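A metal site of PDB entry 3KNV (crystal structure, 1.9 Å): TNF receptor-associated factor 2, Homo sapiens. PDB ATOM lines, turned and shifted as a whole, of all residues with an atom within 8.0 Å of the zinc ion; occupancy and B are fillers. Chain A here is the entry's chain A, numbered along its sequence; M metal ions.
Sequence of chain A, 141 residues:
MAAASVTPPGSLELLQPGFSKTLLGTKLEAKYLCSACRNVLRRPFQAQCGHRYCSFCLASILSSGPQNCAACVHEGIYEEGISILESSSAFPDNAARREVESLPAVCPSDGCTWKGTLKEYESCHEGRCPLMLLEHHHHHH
O of Cys 72 lies within hydrogen-bond range of N of Ile 77 (2.9 Å).
The side-chain carboxylate (OE1) of Glu 75 lies within hydrogen-bond range of a ring nitrogen (NE2) of His 51 (2.8 Å).
SG of Cys 69 sits close to OH of Tyr 53 (3.1 Å).
SG of Cys 72 lies close to OG of Ser 83, at 3.1 Å.
N of Ala 71 lies close to SG of Cys 69.
The backbone carbonyl oxygen (O) of Cys 72 lies within hydrogen-bond range of the backbone NH (N) of Tyr 78, at 3.3 Å.
O of Ser 83 lies within hydrogen-bond range of N of Cys 69, at 2.8 Å.
O of Ile 82 lies within hydrogen-bond range of N of Cys 49 (3.4 Å).
Within 4 Å of the zinc ion: Cys 49, His 51, Cys 69 and Cys 72.
The zinc ion is bound by ND1 of His 51 (2.2 Å).
The side-chain sulfur (SG) of Cys 69 binds the zinc ion (2.3 Å).
The zinc ion is bound by SG of Cys 72 (2.4 Å).
SG of Cys 49 binds the zinc ion.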
ATOM      1  N   SER A  35      15.430 -24.323 -16.938  1.00  0.00           N
ATOM      2  CA  SER A  35      14.755 -23.544 -15.905  1.00  0.00           C
ATOM      3  C   SER A  35      15.738 -22.741 -15.062  1.00  0.00           C
ATOM      4  O   SER A  35      15.352 -21.824 -14.330  1.00  0.00           O
ATOM      5  CB  SER A  35      13.950 -24.468 -15.001  1.00  0.00           C
ATOM      6  OG  SER A  35      12.977 -25.178 -15.743  1.00  0.00           O
ATOM      7  N   ALA A  47      12.772 -32.577 -13.205  1.00  0.00           N
ATOM      8  CA  ALA A  47      12.563 -32.679 -11.764  1.00  0.00           C
ATOM      9  C   ALA A  47      11.159 -33.244 -11.536  1.00  0.00           C
ATOM     10  O   ALA A  47      10.371 -33.366 -12.465  1.00  0.00           O
ATOM     11  CB  ALA A  47      12.692 -31.296 -11.117  1.00  0.00           C
ATOM     12  N   GLN A  48      10.859 -33.594 -10.291  1.00  0.00           N
ATOM     13  CA  GLN A  48       9.569 -34.172  -9.934  1.00  0.00           C
ATOM     14  C   GLN A  48       8.397 -33.280 -10.347  1.00  0.00           C
ATOM     15  O   GLN A  48       7.319 -33.770 -10.693  1.00  0.00           O
ATOM     16  CB  GLN A  48       9.526 -34.431  -8.423  1.00  0.00           C
ATOM     17  CG  GLN A  48       8.203 -34.977  -7.912  1.00  0.00           C
ATOM     18  CD  GLN A  48       8.319 -35.434  -6.467  1.00  0.00           C
ATOM     19  OE1 GLN A  48       8.891 -34.747  -5.623  1.00  0.00           O
ATOM     20  NE2 GLN A  48       7.761 -36.610  -6.179  1.00  0.00           N
ATOM     21  N   CYS A  49       8.612 -31.972 -10.313  1.00  0.00           N
ATOM     22  CA  CYS A  49       7.598 -30.996 -10.677  1.00  0.00           C
ATOM     23  C   CYS A  49       7.345 -30.887 -12.174  1.00  0.00           C
ATOM     24  O   CYS A  49       6.317 -30.349 -12.607  1.00  0.00           O
ATOM     25  CB  CYS A  49       7.998 -29.626 -10.150  1.00  0.00           C
ATOM     26  SG  CYS A  49       9.644 -29.118 -10.722  1.00  0.00           S
ATOM     27  N   GLY A  50       8.284 -31.370 -12.971  1.00  0.00           N
ATOM     28  CA  GLY A  50       8.127 -31.312 -14.412  1.00  0.00           C
ATOM     29  C   GLY A  50       9.066 -30.327 -15.080  1.00  0.00           C
ATOM     30  O   GLY A  50       9.234 -30.361 -16.301  1.00  0.00           O
ATOM     31  N   HIS A  51       9.674 -29.439 -14.302  1.00  0.00           N
ATOM     32  CA  HIS A  51      10.585 -28.461 -14.883  1.00  0.00           C
ATOM     33  C   HIS A  51      11.897 -29.114 -15.305  1.00  0.00           C
ATOM     34  O   HIS A  51      12.426 -29.983 -14.611  1.00  0.00           O
ATOM     35  CB  HIS A  51      10.853 -27.308 -13.901  1.00  0.00           C
ATOM     36  CG  HIS A  51       9.739 -26.299 -13.850  1.00  0.00           C
ATOM     37  ND1 HIS A  51       8.952 -26.112 -12.739  1.00  0.00           N
ATOM     38  CD2 HIS A  51       9.273 -25.443 -14.795  1.00  0.00           C
ATOM     39  CE1 HIS A  51       8.049 -25.178 -12.998  1.00  0.00           C
ATOM     40  NE2 HIS A  51       8.217 -24.772 -14.240  1.00  0.00           N
ATOM     41  N   ARG A  52      12.429 -28.697 -16.437  1.00  0.00           N
ATOM     42  CA  ARG A  52      13.657 -29.266 -16.954  1.00  0.00           C
ATOM     43  C   ARG A  52      14.884 -28.399 -16.679  1.00  0.00           C
ATOM     44  O   ARG A  52      14.807 -27.165 -16.674  1.00  0.00           O
ATOM     45  CB  ARG A  52      13.525 -29.501 -18.455  1.00  0.00           C
ATOM     46  CG  ARG A  52      12.293 -30.317 -18.837  1.00  0.00           C
ATOM     47  CD  ARG A  52      12.249 -30.552 -20.335  1.00  0.00           C
ATOM     48  NE  ARG A  52      11.150 -31.432 -20.732  1.00  0.00           N
ATOM     49  CZ  ARG A  52       9.925 -31.028 -21.036  1.00  0.00           C
ATOM     50  NH1 ARG A  52       9.613 -29.740 -20.997  1.00  0.00           N
ATOM     51  NH2 ARG A  52       9.012 -31.919 -21.401  1.00  0.00           N
ATOM     52  N   TYR A  53      16.011 -29.067 -16.446  1.00  0.00           N
ATOM     53  CA  TYR A  53      17.277 -28.394 -16.160  1.00  0.00           C
ATOM     54  C   TYR A  53      18.415 -29.112 -16.871  1.00  0.00           C
ATOM     55  O   TYR A  53      18.356 -30.329 -17.061  1.00  0.00           O
ATOM     56  CB  TYR A  53      17.596 -28.454 -14.671  1.00  0.00           C
ATOM     57  CG  TYR A  53      16.662 -27.684 -13.770  1.00  0.00           C
ATOM     58  CD1 TYR A  53      15.398 -28.180 -13.450  1.00  0.00           C
ATOM     59  CD2 TYR A  53      17.065 -26.470 -13.220  1.00  0.00           C
ATOM     60  CE1 TYR A  53      14.548 -27.467 -12.594  1.00  0.00           C
ATOM     61  CE2 TYR A  53      16.235 -25.757 -12.378  1.00  0.00           C
ATOM     62  CZ  TYR A  53      14.983 -26.259 -12.062  1.00  0.00           C
ATOM     63  OH  TYR A  53      14.167 -25.530 -11.221  1.00  0.00           O
ATOM     64  N   ASN A  68      14.354 -25.621  -3.334  1.00  0.00           N
ATOM     65  CA  ASN A  68      13.042 -25.343  -3.891  1.00  0.00           C
ATOM     66  C   ASN A  68      13.213 -24.978  -5.355  1.00  0.00           C
ATOM     67  O   ASN A  68      14.154 -24.280  -5.728  1.00  0.00           O
ATOM     68  CB  ASN A  68      12.362 -24.192  -3.154  1.00  0.00           C
ATOM     69  CG  ASN A  68      11.832 -24.600  -1.784  1.00  0.00           C
ATOM     70  OD1 ASN A  68      11.294 -25.689  -1.623  1.00  0.00           O
ATOM     71  ND2 ASN A  68      11.982 -23.720  -0.809  1.00  0.00           N
ATOM     72  N   CYS A  69      12.302 -25.451  -6.186  1.00  0.00           N
ATOM     73  CA  CYS A  69      12.357 -25.160  -7.613  1.00  0.00           C
ATOM     74  C   CYS A  69      11.974 -23.704  -7.848  1.00  0.00           C
ATOM     75  O   CYS A  69      10.818 -23.320  -7.634  1.00  0.00           O
ATOM     76  CB  CYS A  69      11.409 -26.072  -8.385  1.00  0.00           C
ATOM     77  SG  CYS A  69      11.317 -25.657 -10.127  1.00  0.00           S
ATOM     78  N   ALA A  70      12.936 -22.897  -8.285  1.00  0.00           N
ATOM     79  CA  ALA A  70      12.697 -21.479  -8.544  1.00  0.00           C
ATOM     80  C   ALA A  70      11.670 -21.255  -9.650  1.00  0.00           C
ATOM     81  O   ALA A  70      10.909 -20.290  -9.627  1.00  0.00           O
ATOM     82  CB  ALA A  70      14.013 -20.781  -8.902  1.00  0.00           C
ATOM     83  N   ALA A  71      11.651 -22.161 -10.625  1.00  0.00           N
ATOM     84  CA  ALA A  71      10.703 -22.048 -11.730  1.00  0.00           C
ATOM     85  C   ALA A  71       9.276 -22.241 -11.228  1.00  0.00           C
ATOM     86  O   ALA A  71       8.357 -21.542 -11.654  1.00  0.00           O
ATOM     87  CB  ALA A  71      11.019 -23.088 -12.810  1.00  0.00           C
ATOM     88  N   CYS A  72       9.086 -23.191 -10.311  1.00  0.00           N
ATOM     89  CA  CYS A  72       7.759 -23.421  -9.752  1.00  0.00           C
ATOM     90  C   CYS A  72       7.284 -22.165  -9.035  1.00  0.00           C
ATOM     91  O   CYS A  72       6.148 -21.718  -9.219  1.00  0.00           O
ATOM     92  CB  CYS A  72       7.794 -24.593  -8.764  1.00  0.00           C
ATOM     93  SG  CYS A  72       7.483 -26.219  -9.473  1.00  0.00           S
ATOM     94  N   VAL A  73       8.177 -21.584  -8.239  1.00  0.00           N
ATOM     95  CA  VAL A  73       7.868 -20.377  -7.501  1.00  0.00           C
ATOM     96  C   VAL A  73       7.453 -19.242  -8.434  1.00  0.00           C
ATOM     97  O   VAL A  73       6.341 -18.721  -8.337  1.00  0.00           O
ATOM     98  CB  VAL A  73       9.084 -19.904  -6.682  1.00  0.00           C
ATOM     99  CG1 VAL A  73       8.783 -18.576  -5.993  1.00  0.00           C
ATOM    100  CG2 VAL A  73       9.444 -20.971  -5.647  1.00  0.00           C
ATOM    101  N   GLU A  75       6.514 -19.254 -11.447  1.00  0.00           N
ATOM    102  CA  GLU A  75       5.322 -19.560 -12.231  1.00  0.00           C
ATOM    103  C   GLU A  75       4.091 -19.685 -11.351  1.00  0.00           C
ATOM    104  O   GLU A  75       2.994 -19.924 -11.849  1.00  0.00           O
ATOM    105  CB  GLU A  75       5.525 -20.851 -13.029  1.00  0.00           C
ATOM    106  CG  GLU A  75       6.198 -20.620 -14.377  1.00  0.00           C
ATOM    107  CD  GLU A  75       6.858 -21.860 -14.925  1.00  0.00           C
ATOM    108  OE1 GLU A  75       6.240 -22.942 -14.901  1.00  0.00           O
ATOM    109  OE2 GLU A  75       8.006 -21.749 -15.399  1.00  0.00           O
ATOM    110  N   ILE A  77       3.259 -21.995  -9.100  1.00  0.00           N
ATOM    111  CA  ILE A  77       2.696 -23.334  -8.994  1.00  0.00           C
ATOM    112  C   ILE A  77       3.450 -24.170  -7.973  1.00  0.00           C
ATOM    113  O   ILE A  77       3.298 -25.384  -7.917  1.00  0.00           O
ATOM    114  CB  ILE A  77       2.721 -24.049 -10.356  1.00  0.00           C
ATOM    115  CG1 ILE A  77       4.155 -24.121 -10.890  1.00  0.00           C
ATOM    116  CG2 ILE A  77       1.834 -23.303 -11.349  1.00  0.00           C
ATOM    117  CD1 ILE A  77       4.263 -24.817 -12.237  1.00  0.00           C
ATOM    118  N   TYR A  78       4.255 -23.498  -7.148  1.00  0.00           N
ATOM    119  CA  TYR A  78       5.021 -24.177  -6.122  1.00  0.00           C
ATOM    120  C   TYR A  78       4.111 -24.980  -5.213  1.00  0.00           C
ATOM    121  O   TYR A  78       3.105 -24.475  -4.708  1.00  0.00           O
ATOM    122  CB  TYR A  78       5.794 -23.177  -5.253  1.00  0.00           C
ATOM    123  CG  TYR A  78       6.559 -23.843  -4.133  1.00  0.00           C
ATOM    124  CD1 TYR A  78       7.825 -24.389  -4.357  1.00  0.00           C
ATOM    125  CD2 TYR A  78       5.994 -23.971  -2.868  1.00  0.00           C
ATOM    126  CE1 TYR A  78       8.505 -25.047  -3.331  1.00  0.00           C
ATOM    127  CE2 TYR A  78       6.675 -24.629  -1.842  1.00  0.00           C
ATOM    128  CZ  TYR A  78       7.933 -25.164  -2.084  1.00  0.00           C
ATOM    129  OH  TYR A  78       8.591 -25.827  -1.075  1.00  0.00           O
ATOM    130  N   GLU A  79       4.465 -26.253  -5.023  1.00  0.00           N
ATOM    131  CA  GLU A  79       3.697 -27.154  -4.165  1.00  0.00           C
ATOM    132  C   GLU A  79       4.697 -27.899  -3.287  1.00  0.00           C
ATOM    133  O   GLU A  79       5.672 -28.452  -3.771  1.00  0.00           O
ATOM    134  CB  GLU A  79       2.902 -28.145  -5.008  1.00  0.00           C
ATOM    135  CG  GLU A  79       1.806 -27.521  -5.848  1.00  0.00           C
ATOM    136  CD  GLU A  79       1.112 -28.516  -6.753  1.00  0.00           C
ATOM    137  OE1 GLU A  79       0.184 -28.098  -7.488  1.00  0.00           O
ATOM    138  OE2 GLU A  79       1.481 -29.707  -6.732  1.00  0.00           O
ATOM    139  N   ILE A  82       6.483 -31.776  -3.954  1.00  0.00           N
ATOM    140  CA  ILE A  82       6.627 -31.916  -5.399  1.00  0.00           C
ATOM    141  C   ILE A  82       7.538 -30.882  -6.045  1.00  0.00           C
ATOM    142  O   ILE A  82       8.248 -31.193  -7.001  1.00  0.00           O
ATOM    143  CB  ILE A  82       5.237 -31.893  -6.083  1.00  0.00           C
ATOM    144  CG1 ILE A  82       4.669 -33.318  -6.160  1.00  0.00           C
ATOM    145  CG2 ILE A  82       5.324 -31.302  -7.482  1.00  0.00           C
ATOM    146  CD1 ILE A  82       4.549 -34.009  -4.816  1.00  0.00           C
ATOM    147  N   SER A  83       7.536 -29.655  -5.523  1.00  0.00           N
ATOM    148  CA  SER A  83       8.361 -28.594  -6.086  1.00  0.00           C
ATOM    149  C   SER A  83       9.752 -28.515  -5.473  1.00  0.00           C
ATOM    150  O   SER A  83      10.425 -27.485  -5.566  1.00  0.00           O
ATOM    151  CB  SER A  83       7.648 -27.251  -5.947  1.00  0.00           C
ATOM    152  OG  SER A  83       6.457 -27.212  -6.711  1.00  0.00           O
ATOM    153  N   ILE A  84      10.196 -29.600  -4.848  1.00  0.00           N
ATOM    154  CA  ILE A  84      11.522 -29.631  -4.245  1.00  0.00           C
ATOM    155  C   ILE A  84      12.477 -30.403  -5.150  1.00  0.00           C
ATOM    156  O   ILE A  84      12.268 -31.584  -5.428  1.00  0.00           O
ATOM    157  CB  ILE A  84      11.504 -30.351  -2.885  1.00  0.00           C
ATOM    158  CG1 ILE A  84      10.336 -29.855  -2.049  1.00  0.00           C
ATOM    159  CG2 ILE A  84      12.837 -30.119  -2.170  1.00  0.00           C
ATOM    160  CD1 ILE A  84      10.325 -28.371  -1.803  1.00  0.00           C
ATOM    161  N   LEU A  85      13.535 -29.730  -5.612  1.00  0.00           N
ATOM    162  CA  LEU A  85      14.523 -30.379  -6.469  1.00  0.00           C
ATOM    163  C   LEU A  85      15.330 -31.356  -5.620  1.00  0.00           C
ATOM    164  O   LEU A  85      15.929 -30.962  -4.619  1.00  0.00           O
ATOM    165  CB  LEU A  85      15.451 -29.322  -7.085  1.00  0.00           C
ATOM    166  CG  LEU A  85      14.742 -28.219  -7.879  1.00  0.00           C
ATOM    167  CD1 LEU A  85      15.751 -27.223  -8.417  1.00  0.00           C
ATOM    168  CD2 LEU A  85      13.960 -28.861  -9.034  1.00  0.00           C
HETATM  169 ZN    ZN M   1       9.406 -26.767 -10.730  1.00  0.00          ZN
